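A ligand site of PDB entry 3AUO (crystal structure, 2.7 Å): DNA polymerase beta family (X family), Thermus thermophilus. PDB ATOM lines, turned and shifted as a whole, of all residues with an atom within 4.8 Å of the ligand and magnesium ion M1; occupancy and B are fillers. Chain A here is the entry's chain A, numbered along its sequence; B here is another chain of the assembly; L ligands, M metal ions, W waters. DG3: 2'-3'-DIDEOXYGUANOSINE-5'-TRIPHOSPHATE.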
ATOM      1  N   ARG A  35      19.104  13.762  26.240  1.00  0.00           N
ATOM      2  CA  ARG A  35      19.272  12.689  25.254  1.00  0.00           C
ATOM      3  C   ARG A  35      17.934  12.079  24.830  1.00  0.00           C
ATOM      4  O   ARG A  35      17.744  11.741  23.655  1.00  0.00           O
ATOM      5  CB  ARG A  35      20.208  11.606  25.818  1.00  0.00           C
ATOM      6  CG  ARG A  35      20.451  10.408  24.890  1.00  0.00           C
ATOM      7  CD  ARG A  35      21.137  10.815  23.592  1.00  0.00           C
ATOM      8  NE  ARG A  35      21.652   9.657  22.862  1.00  0.00           N
ATOM      9  CZ  ARG A  35      22.485   9.711  21.814  1.00  0.00           C
ATOM     10  NH1 ARG A  35      22.907  10.878  21.338  1.00  0.00           N
ATOM     11  NH2 ARG A  35      22.890   8.592  21.236  1.00  0.00           N
ATOM     12  N   ARG A 157      25.988  13.778  13.188  1.00  0.00           N
ATOM     13  CA  ARG A 157      25.620  12.373  13.196  1.00  0.00           C
ATOM     14  C   ARG A 157      25.202  12.032  11.764  1.00  0.00           C
ATOM     15  O   ARG A 157      24.695  12.899  11.056  1.00  0.00           O
ATOM     16  CB  ARG A 157      24.453  12.110  14.155  1.00  0.00           C
ATOM     17  CG  ARG A 157      24.705  12.537  15.601  1.00  0.00           C
ATOM     18  CD  ARG A 157      23.459  12.318  16.454  1.00  0.00           C
ATOM     19  NE  ARG A 157      22.986  10.942  16.343  1.00  0.00           N
ATOM     20  CZ  ARG A 157      23.518   9.906  16.985  1.00  0.00           C
ATOM     21  NH1 ARG A 157      24.548  10.049  17.803  1.00  0.00           N
ATOM     22  NH2 ARG A 157      22.996   8.688  16.806  1.00  0.00           N
ATOM     23  N   GLY A 187      27.120  -0.939  19.110  1.00  0.00           N
ATOM     24  CA  GLY A 187      26.674   0.429  19.272  1.00  0.00           C
ATOM     25  C   GLY A 187      25.276   0.636  18.714  1.00  0.00           C
ATOM     26  O   GLY A 187      24.488  -0.307  18.637  1.00  0.00           O
ATOM     27  N   SER A 188      24.984   1.870  18.301  1.00  0.00           N
ATOM     28  CA  SER A 188      23.677   2.223  17.767  1.00  0.00           C
ATOM     29  C   SER A 188      23.369   1.523  16.440  1.00  0.00           C
ATOM     30  O   SER A 188      22.197   1.295  16.108  1.00  0.00           O
ATOM     31  CB  SER A 188      23.588   3.748  17.603  1.00  0.00           C
ATOM     32  OG  SER A 188      24.800   4.247  17.062  1.00  0.00           O
ATOM     33  N   ARG A 191      21.453  -1.559  16.944  1.00  0.00           N
ATOM     34  CA  ARG A 191      20.090  -1.272  17.413  1.00  0.00           C
ATOM     35  C   ARG A 191      19.247  -0.601  16.325  1.00  0.00           C
ATOM     36  O   ARG A 191      18.106  -0.220  16.581  1.00  0.00           O
ATOM     37  CB  ARG A 191      20.135  -0.338  18.636  1.00  0.00           C
ATOM     38  CG  ARG A 191      21.159  -0.731  19.699  1.00  0.00           C
ATOM     39  CD  ARG A 191      20.840  -0.073  21.033  1.00  0.00           C
ATOM     40  NE  ARG A 191      20.762   1.388  20.959  1.00  0.00           N
ATOM     41  CZ  ARG A 191      21.806   2.205  20.970  1.00  0.00           C
ATOM     42  NH1 ARG A 191      23.047   1.743  21.043  1.00  0.00           N
ATOM     43  NH2 ARG A 191      21.611   3.521  20.896  1.00  0.00           N
ATOM     44  N   LYS A 193      19.277   2.324  15.129  1.00  0.00           N
ATOM     45  CA  LYS A 193      18.996   3.743  15.358  1.00  0.00           C
ATOM     46  C   LYS A 193      19.116   4.467  14.027  1.00  0.00           C
ATOM     47  O   LYS A 193      20.099   4.284  13.316  1.00  0.00           O
ATOM     48  CB  LYS A 193      19.979   4.306  16.380  1.00  0.00           C
ATOM     49  CG  LYS A 193      19.646   5.681  16.964  1.00  0.00           C
ATOM     50  CD  LYS A 193      20.689   6.048  18.014  1.00  0.00           C
ATOM     51  CE  LYS A 193      20.629   7.505  18.439  1.00  0.00           C
ATOM     52  NZ  LYS A 193      19.528   7.753  19.398  1.00  0.00           N
ATOM     53  N   THR A 195      19.998   7.265  12.951  1.00  0.00           N
ATOM     54  CA  THR A 195      21.286   7.918  12.741  1.00  0.00           C
ATOM     55  C   THR A 195      22.291   7.400  13.747  1.00  0.00           C
ATOM     56  O   THR A 195      21.907   6.936  14.819  1.00  0.00           O
ATOM     57  CB  THR A 195      21.204   9.441  12.928  1.00  0.00           C
ATOM     58  OG1 THR A 195      20.957   9.742  14.305  1.00  0.00           O
ATOM     59  CG2 THR A 195      20.100  10.035  12.053  1.00  0.00           C
ATOM     60  N   VAL A 196      23.572   7.490  13.399  1.00  0.00           N
ATOM     61  CA  VAL A 196      24.652   7.096  14.299  1.00  0.00           C
ATOM     62  C   VAL A 196      25.649   8.229  14.511  1.00  0.00           C
ATOM     63  O   VAL A 196      25.844   9.064  13.629  1.00  0.00           O
ATOM     64  CB  VAL A 196      25.413   5.874  13.752  1.00  0.00           C
ATOM     65  CG1 VAL A 196      24.431   4.765  13.395  1.00  0.00           C
ATOM     66  CG2 VAL A 196      26.242   6.259  12.539  1.00  0.00           C
ATOM     67  N   GLY A 197      26.263   8.252  15.694  1.00  0.00           N
ATOM     68  CA  GLY A 197      27.350   9.174  15.998  1.00  0.00           C
ATOM     69  C   GLY A 197      28.713   8.641  15.569  1.00  0.00           C
ATOM     70  O   GLY A 197      29.661   9.408  15.415  1.00  0.00           O
ATOM     71  N   ASP A 198      28.816   7.325  15.389  1.00  0.00           N
ATOM     72  CA  ASP A 198      30.063   6.676  14.982  1.00  0.00           C
ATOM     73  C   ASP A 198      29.756   5.230  14.597  1.00  0.00           C
ATOM     74  O   ASP A 198      28.587   4.876  14.445  1.00  0.00           O
ATOM     75  CB  ASP A 198      31.082   6.711  16.132  1.00  0.00           C
ATOM     76  CG  ASP A 198      30.718   5.769  17.281  1.00  0.00           C
ATOM     77  OD1 ASP A 198      29.520   5.508  17.501  1.00  0.00           O
ATOM     78  OD2 ASP A 198      31.648   5.301  17.972  1.00  0.00           O
ATOM     79  N   ASP A 200      30.798   1.351  16.156  1.00  0.00           N
ATOM     80  CA  ASP A 200      31.403   0.715  17.328  1.00  0.00           C
ATOM     81  C   ASP A 200      31.586  -0.782  17.113  1.00  0.00           C
ATOM     82  O   ASP A 200      30.616  -1.544  17.146  1.00  0.00           O
ATOM     83  CB  ASP A 200      30.512   0.928  18.553  1.00  0.00           C
ATOM     84  CG  ASP A 200      30.247   2.383  18.835  1.00  0.00           C
ATOM     85  OD1 ASP A 200      31.109   3.044  19.452  1.00  0.00           O
ATOM     86  OD2 ASP A 200      29.154   2.868  18.467  1.00  0.00           O
ATOM     87  N   TYR A 258      27.883  -4.824  26.469  1.00  0.00           N
ATOM     88  CA  TYR A 258      28.505  -3.543  26.811  1.00  0.00           C
ATOM     89  C   TYR A 258      28.536  -2.572  25.640  1.00  0.00           C
ATOM     90  O   TYR A 258      28.063  -1.440  25.761  1.00  0.00           O
ATOM     91  CB  TYR A 258      29.926  -3.728  27.336  1.00  0.00           C
ATOM     92  CG  TYR A 258      30.722  -2.437  27.312  1.00  0.00           C
ATOM     93  CD1 TYR A 258      30.401  -1.377  28.148  1.00  0.00           C
ATOM     94  CD2 TYR A 258      31.779  -2.262  26.411  1.00  0.00           C
ATOM     95  CE1 TYR A 258      31.103  -0.186  28.121  1.00  0.00           C
ATOM     96  CE2 TYR A 258      32.489  -1.076  26.381  1.00  0.00           C
ATOM     97  CZ  TYR A 258      32.148  -0.042  27.233  1.00  0.00           C
ATOM     98  OH  TYR A 258      32.860   1.133  27.195  1.00  0.00           O
ATOM     99  N   LEU A 259      29.101  -3.009  24.516  1.00  0.00           N
ATOM    100  CA  LEU A 259      29.286  -2.121  23.360  1.00  0.00           C
ATOM    101  C   LEU A 259      27.998  -1.848  22.590  1.00  0.00           C
ATOM    102  O   LEU A 259      27.920  -0.885  21.850  1.00  0.00           O
ATOM    103  CB  LEU A 259      30.347  -2.667  22.413  1.00  0.00           C
ATOM    104  CG  LEU A 259      31.073  -1.612  21.582  1.00  0.00           C
ATOM    105  CD1 LEU A 259      31.827  -0.629  22.479  1.00  0.00           C
ATOM    106  CD2 LEU A 259      32.019  -2.266  20.589  1.00  0.00           C
ATOM    107  N   THR A 260      26.987  -2.694  22.759  1.00  0.00           N
ATOM    108  CA  THR A 260      25.722  -2.494  22.059  1.00  0.00           C
ATOM    109  C   THR A 260      24.860  -1.436  22.733  1.00  0.00           C
ATOM    110  O   THR A 260      24.196  -0.656  22.057  1.00  0.00           O
ATOM    111  CB  THR A 260      24.957  -3.806  21.917  1.00  0.00           C
ATOM    112  OG1 THR A 260      25.700  -4.696  21.080  1.00  0.00           O
ATOM    113  CG2 THR A 260      23.568  -3.573  21.315  1.00  0.00           C
ATOM    114  N   GLY A 261      24.858  -1.409  24.071  1.00  0.00           N
ATOM    115  CA  GLY A 261      24.078  -0.422  24.804  1.00  0.00           C
ATOM    116  C   GLY A 261      22.592  -0.549  24.518  1.00  0.00           C
ATOM    117  O   GLY A 261      22.126  -1.640  24.210  1.00  0.00           O
ATOM    118  N   SER A 262      21.824   0.531  24.582  1.00  0.00           N
ATOM    119  CA  SER A 262      22.306   1.887  24.866  1.00  0.00           C
ATOM    120  C   SER A 262      22.884   2.082  26.266  1.00  0.00           C
ATOM    121  O   SER A 262      22.661   1.288  27.167  1.00  0.00           O
ATOM    122  CB  SER A 262      21.129   2.850  24.709  1.00  0.00           C
ATOM    123  OG  SER A 262      20.075   2.460  25.586  1.00  0.00           O
ATOM    124  N   LYS A 263      23.620   3.179  26.421  1.00  0.00           N
ATOM    125  CA  LYS A 263      24.060   3.677  27.722  1.00  0.00           C
ATOM    126  C   LYS A 263      22.961   3.486  28.750  1.00  0.00           C
ATOM    127  O   LYS A 263      23.147   2.778  29.735  1.00  0.00           O
ATOM    128  CB  LYS A 263      24.425   5.172  27.582  1.00  0.00           C
ATOM    129  CG  LYS A 263      24.983   5.857  28.826  1.00  0.00           C
ATOM    130  CD  LYS A 263      25.449   7.267  28.485  1.00  0.00           C
ATOM    131  CE  LYS A 263      26.184   7.944  29.639  1.00  0.00           C
ATOM    132  NZ  LYS A 263      25.286   8.216  30.795  1.00  0.00           N
ATOM    133  N   SER A 266      22.037  -0.174  29.322  1.00  0.00           N
ATOM    134  CA  SER A 266      23.169  -0.772  30.032  1.00  0.00           C
ATOM    135  C   SER A 266      23.165  -0.399  31.519  1.00  0.00           C
ATOM    136  O   SER A 266      23.453  -1.253  32.358  1.00  0.00           O
ATOM    137  CB  SER A 266      24.494  -0.331  29.398  1.00  0.00           C
ATOM    138  OG  SER A 266      24.716  -1.006  28.175  1.00  0.00           O
ATOM    139  N   ARG A 270      23.020  -2.883  34.854  1.00  0.00           N
ATOM    140  CA  ARG A 270      24.050  -2.832  35.890  1.00  0.00           C
ATOM    141  C   ARG A 270      23.427  -2.496  37.249  1.00  0.00           C
ATOM    142  O   ARG A 270      23.719  -3.161  38.257  1.00  0.00           O
ATOM    143  CB  ARG A 270      25.156  -1.850  35.499  1.00  0.00           C
ATOM    144  CG  ARG A 270      25.898  -2.323  34.263  1.00  0.00           C
ATOM    145  CD  ARG A 270      27.080  -1.449  33.906  1.00  0.00           C
ATOM    146  NE  ARG A 270      27.767  -2.007  32.742  1.00  0.00           N
ATOM    147  CZ  ARG A 270      29.050  -1.825  32.452  1.00  0.00           C
ATOM    148  NH1 ARG A 270      29.559  -2.404  31.357  1.00  0.00           N
ATOM    149  NH2 ARG A 270      29.838  -1.079  33.219  1.00  0.00           N
ATOM    150  P    DC B  13      24.670   4.536  38.548  1.00  0.00           P
ATOM    151  OP1  DC B  13      25.734   5.550  38.758  1.00  0.00           O
ATOM    152  OP2  DC B  13      23.817   4.602  37.340  1.00  0.00           O
ATOM    153  O5'  DC B  13      25.378   3.106  38.607  1.00  0.00           O
ATOM    154  C5'  DC B  13      24.708   1.930  38.243  1.00  0.00           C
ATOM    155  C4'  DC B  13      25.714   0.899  37.768  1.00  0.00           C
ATOM    156  O4'  DC B  13      26.152   1.260  36.431  1.00  0.00           O
ATOM    157  C3'  DC B  13      26.978   0.789  38.611  1.00  0.00           C
ATOM    158  O3'  DC B  13      27.373  -0.580  38.685  1.00  0.00           O
ATOM    159  C2'  DC B  13      27.974   1.676  37.871  1.00  0.00           C
ATOM    160  C1'  DC B  13      27.528   1.565  36.411  1.00  0.00           C
ATOM    161  N1   DC B  13      27.700   2.799  35.555  1.00  0.00           N
ATOM    162  C2   DC B  13      28.147   2.672  34.224  1.00  0.00           C
ATOM    163  O2   DC B  13      28.402   1.558  33.749  1.00  0.00           O
ATOM    164  N3   DC B  13      28.281   3.793  33.458  1.00  0.00           N
ATOM    165  C4   DC B  13      28.002   4.996  33.963  1.00  0.00           C
ATOM    166  N4   DC B  13      28.152   6.074  33.176  1.00  0.00           N
ATOM    167  C5   DC B  13      27.550   5.146  35.310  1.00  0.00           C
ATOM    168  C6   DC B  13      27.412   4.036  36.048  1.00  0.00           C
ATOM    169  P    DC B  14      28.614  -1.108  39.537  1.00  0.00           P
ATOM    170  OP1  DC B  14      28.356  -2.517  39.883  1.00  0.00           O
ATOM    171  OP2  DC B  14      28.932  -0.137  40.605  1.00  0.00           O
ATOM    172  O5'  DC B  14      29.805  -1.038  38.483  1.00  0.00           O
ATOM    173  C5'  DC B  14      29.794  -1.930  37.405  1.00  0.00           C
ATOM    174  C4'  DC B  14      30.992  -1.647  36.524  1.00  0.00           C
ATOM    175  O4'  DC B  14      30.816  -0.329  35.951  1.00  0.00           O
ATOM    176  C3'  DC B  14      32.356  -1.629  37.228  1.00  0.00           C
ATOM    177  O3'  DC B  14      33.174  -2.654  36.641  1.00  0.00           O
ATOM    178  C2'  DC B  14      32.844  -0.190  37.021  1.00  0.00           C
ATOM    179  C1'  DC B  14      32.109   0.185  35.737  1.00  0.00           C
ATOM    180  N1   DC B  14      31.912   1.624  35.368  1.00  0.00           N
ATOM    181  C2   DC B  14      32.185   2.061  34.060  1.00  0.00           C
ATOM    182  O2   DC B  14      32.628   1.274  33.208  1.00  0.00           O
ATOM    183  N3   DC B  14      31.974   3.351  33.741  1.00  0.00           N
ATOM    184  C4   DC B  14      31.494   4.207  34.645  1.00  0.00           C
ATOM    185  N4   DC B  14      31.316   5.474  34.259  1.00  0.00           N
ATOM    186  C5   DC B  14      31.193   3.789  35.979  1.00  0.00           C
ATOM    187  C6   DC B  14      31.413   2.500  36.286  1.00  0.00           C
ATOM    188  P   DDG B  29      32.924   9.240  23.828  1.00  0.00           P
ATOM    189  OP1 DDG B  29      33.178   9.444  22.344  1.00  0.00           O
ATOM    190  OP2 DDG B  29      31.786   9.932  24.533  1.00  0.00           O
ATOM    191  O5' DDG B  29      32.795   7.641  24.095  1.00  0.00           O
ATOM    192  C5' DDG B  29      33.563   6.723  23.325  1.00  0.00           C
ATOM    193  C4' DDG B  29      33.379   5.280  23.810  1.00  0.00           C
ATOM    194  O4' DDG B  29      33.839   5.133  25.149  1.00  0.00           O
ATOM    195  C3' DDG B  29      31.919   4.824  23.801  1.00  0.00           C
ATOM    196  C2' DDG B  29      31.808   3.922  25.011  1.00  0.00           C
ATOM    197  C1' DDG B  29      32.979   4.282  25.907  1.00  0.00           C
ATOM    198  N9  DDG B  29      32.528   5.007  27.126  1.00  0.00           N
ATOM    199  C8  DDG B  29      32.147   6.299  27.194  1.00  0.00           C
ATOM    200  N7  DDG B  29      31.808   6.635  28.472  1.00  0.00           N
ATOM    201  C5  DDG B  29      31.972   5.550  29.234  1.00  0.00           C
ATOM    202  C6  DDG B  29      31.795   5.200  30.659  1.00  0.00           C
ATOM    203  O6  DDG B  29      31.397   6.034  31.498  1.00  0.00           O
ATOM    204  N1  DDG B  29      32.081   3.936  31.037  1.00  0.00           N
ATOM    205  C2  DDG B  29      32.505   3.002  30.161  1.00  0.00           C
ATOM    206  N2  DDG B  29      32.774   1.752  30.599  1.00  0.00           N
ATOM    207  N3  DDG B  29      32.696   3.252  28.848  1.00  0.00           N
ATOM    208  C4  DDG B  29      32.445   4.477  28.341  1.00  0.00           C
HETATM  209  PG  DG3 L   1      25.922   6.857  18.935  1.00  0.00           P
HETATM  210  O1G DG3 L   1      27.355   6.417  18.941  1.00  0.00           O
HETATM  211  O2G DG3 L   1      25.728   8.252  19.474  1.00  0.00           O
HETATM  212  O3G DG3 L   1      25.213   6.636  17.638  1.00  0.00           O
HETATM  213  O3B DG3 L   1      25.156   5.880  19.950  1.00  0.00           O
HETATM  214  PB  DG3 L   1      25.880   4.675  20.731  1.00  0.00           P
HETATM  215  O1B DG3 L   1      24.833   4.011  21.577  1.00  0.00           O
HETATM  216  O2B DG3 L   1      26.644   3.820  19.746  1.00  0.00           O
HETATM  217  O3A DG3 L   1      26.888   5.464  21.711  1.00  0.00           O
HETATM  218  PA  DG3 L   1      28.503   5.353  21.744  1.00  0.00           P
HETATM  219  O1A DG3 L   1      29.013   4.949  20.381  1.00  0.00           O
HETATM  220  O2A DG3 L   1      28.980   6.611  22.418  1.00  0.00           O
HETATM  221  O5' DG3 L   1      28.855   4.142  22.753  1.00  0.00           O
HETATM  222  C5' DG3 L   1      28.948   2.814  22.262  1.00  0.00           C
HETATM  223  C4' DG3 L   1      28.572   1.808  23.351  1.00  0.00           C
HETATM  224  O4' DG3 L   1      29.282   2.049  24.562  1.00  0.00           O
HETATM  225  C3' DG3 L   1      27.088   1.860  23.664  1.00  0.00           C
HETATM  226  C2' DG3 L   1      26.989   1.764  25.171  1.00  0.00           C
HETATM  227  C1' DG3 L   1      28.411   1.894  25.684  1.00  0.00           C
HETATM  228  N9  DG3 L   1      28.519   3.066  26.587  1.00  0.00           N
HETATM  229  C8  DG3 L   1      28.605   4.364  26.242  1.00  0.00           C
HETATM  230  N7  DG3 L   1      28.678   5.153  27.343  1.00  0.00           N
HETATM  231  C5  DG3 L   1      28.620   4.356  28.419  1.00  0.00           C
HETATM  232  C6  DG3 L   1      28.639   4.516  29.896  1.00  0.00           C
HETATM  233  O6  DG3 L   1      28.723   5.654  30.396  1.00  0.00           O
HETATM  234  N1  DG3 L   1      28.562   3.415  30.654  1.00  0.00           N
HETATM  235  C2  DG3 L   1      28.457   2.193  30.128  1.00  0.00           C
HETATM  236  N2  DG3 L   1      28.371   1.107  30.934  1.00  0.00           N
HETATM  237  N3  DG3 L   1      28.430   1.958  28.795  1.00  0.00           N
HETATM  238  C4  DG3 L   1      28.512   2.982  27.915  1.00  0.00           C
HETATM  239 MG    MG M   1      27.951   4.505  18.519  1.00  0.00          MG
HETATM  240 MG    MG M   2      31.524   5.871  20.510  1.00  0.00          MG
HETATM  241  O   HOH W   1      27.416  -0.454  28.053  1.00  0.00           O
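Magnesium ion M1 is bound by an oxygen (O2B) of the ligand (1.9 Å), the side-chain carboxylate (OD2) of Asp 200 (2.0 Å), an oxygen (O1G) of the ligand (2.0 Å), the side-chain carboxylate (OD1) of Asp 198 (2.1 Å) and an oxygen (O1A) of the ligand (2.2 Å).
Magnesium ion M1 has five donor atoms within binding distance.
The backbone carbonyl oxygen (O) of Ser 188 sits at hydrogen-bond distance from the backbone NH (N) of Lys 193, 3.2 Å away.
The backbone carbonyl oxygen (O) of Thr 195 sits at hydrogen-bond distance from the guanidinium group (NH2) of Arg 157 (2.9 Å).
O2 of DC 13 of chain B is in hydrogen-bond range of NH2 of Arg 270 (3.0 Å).
N3 of DDG 29 of chain B lies within hydrogen-bond range of OH of Tyr 258, at 2.7 Å.
N2 of DDG 29 of chain B lies close to O2 of DC 14 of chain B (2.7 Å).
The backbone carbonyl oxygen (O) of Gly 187 lies close to the guanidinium group (NH1) of Arg 191 (3.5 Å).
The guanidinium group of Arg 191 is in hydrogen-bond range of the backbone carbonyl oxygen of Thr 260, 2.8 Å away.
The backbone carbonyl oxygen (O) of Leu 259 is in hydrogen-bond range of the backbone NH (N) of Gly 187, 2.9 Å away.
OG of Ser 188 touches magnesium ion M1, at 3.5 Å.
The nearest printed residue that does not touch magnesium ion M1 is Gly 187 (4.3 Å).
An oxygen (O2B) of the ligand sits close to the backbone NH (N) of Ser 188 (2.9 Å).
An oxygen (O3G) of the ligand is in hydrogen-bond range of the side-chain hydroxyl of Ser 188 (2.5 Å).
The guanidinium group (NH1) of Arg 157 lies within salt-bridge range of an oxygen (O2G) of the ligand, at 2.7 Å.
An oxygen (O3G) of the ligand lies within hydrogen-bond range of the backbone NH (N) of Gly 197, at 2.7 Å.
N3 of DC 13 of chain B is in hydrogen-bond range of a nitrogen (N1) of the ligand (2.8 Å).
The guanidinium group (NH1) of Arg 191 lies within salt-bridge range of an oxygen (O1B) of the ligand, at 2.9 Å.
An oxygen (O2G) of the ligand lies within salt-bridge range of the guanidinium group (NH2) of Arg 35 (3.4 Å).
Water W1 lies within hydrogen-bond range of O of Tyr 258 (2.6 Å), N3 of the ligand (2.7 Å) and OG of Ser 266 (2.8 Å).
A nitrogen (N2) of the ligand sits close to the guanidinium group (NH2) of Arg 270, at 3.5 Å.
O6 of DDG 29 of chain B sits close to O6 of the ligand (2.9 Å).
Gly 187 touches the ligand.
Val 196 touches the ligand.
Tyr 258 touches the ligand (O to C1', 3.4 Å).
Leu 259 touches the ligand (O to C4', 3.2 Å).
CA of Gly 261 touches C2' of the ligand, 3.7 Å away.
Lys 263 touches the ligand (CE to O6, 3.5 Å).
Hydrophobic or aromatic side chains within 4 Å of the ligand: Val 196 and Tyr 258.
Within 4 Å of the ligand: Arg 35, Arg 157, Gly 187, Ser 188, Arg 191, Val 196, Gly 197, Asp 198, Asp 200, Tyr 258, Leu 259, Gly 261, Lys 263, Arg 270, DC 13 of chain B and DDG 29 of chain B.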
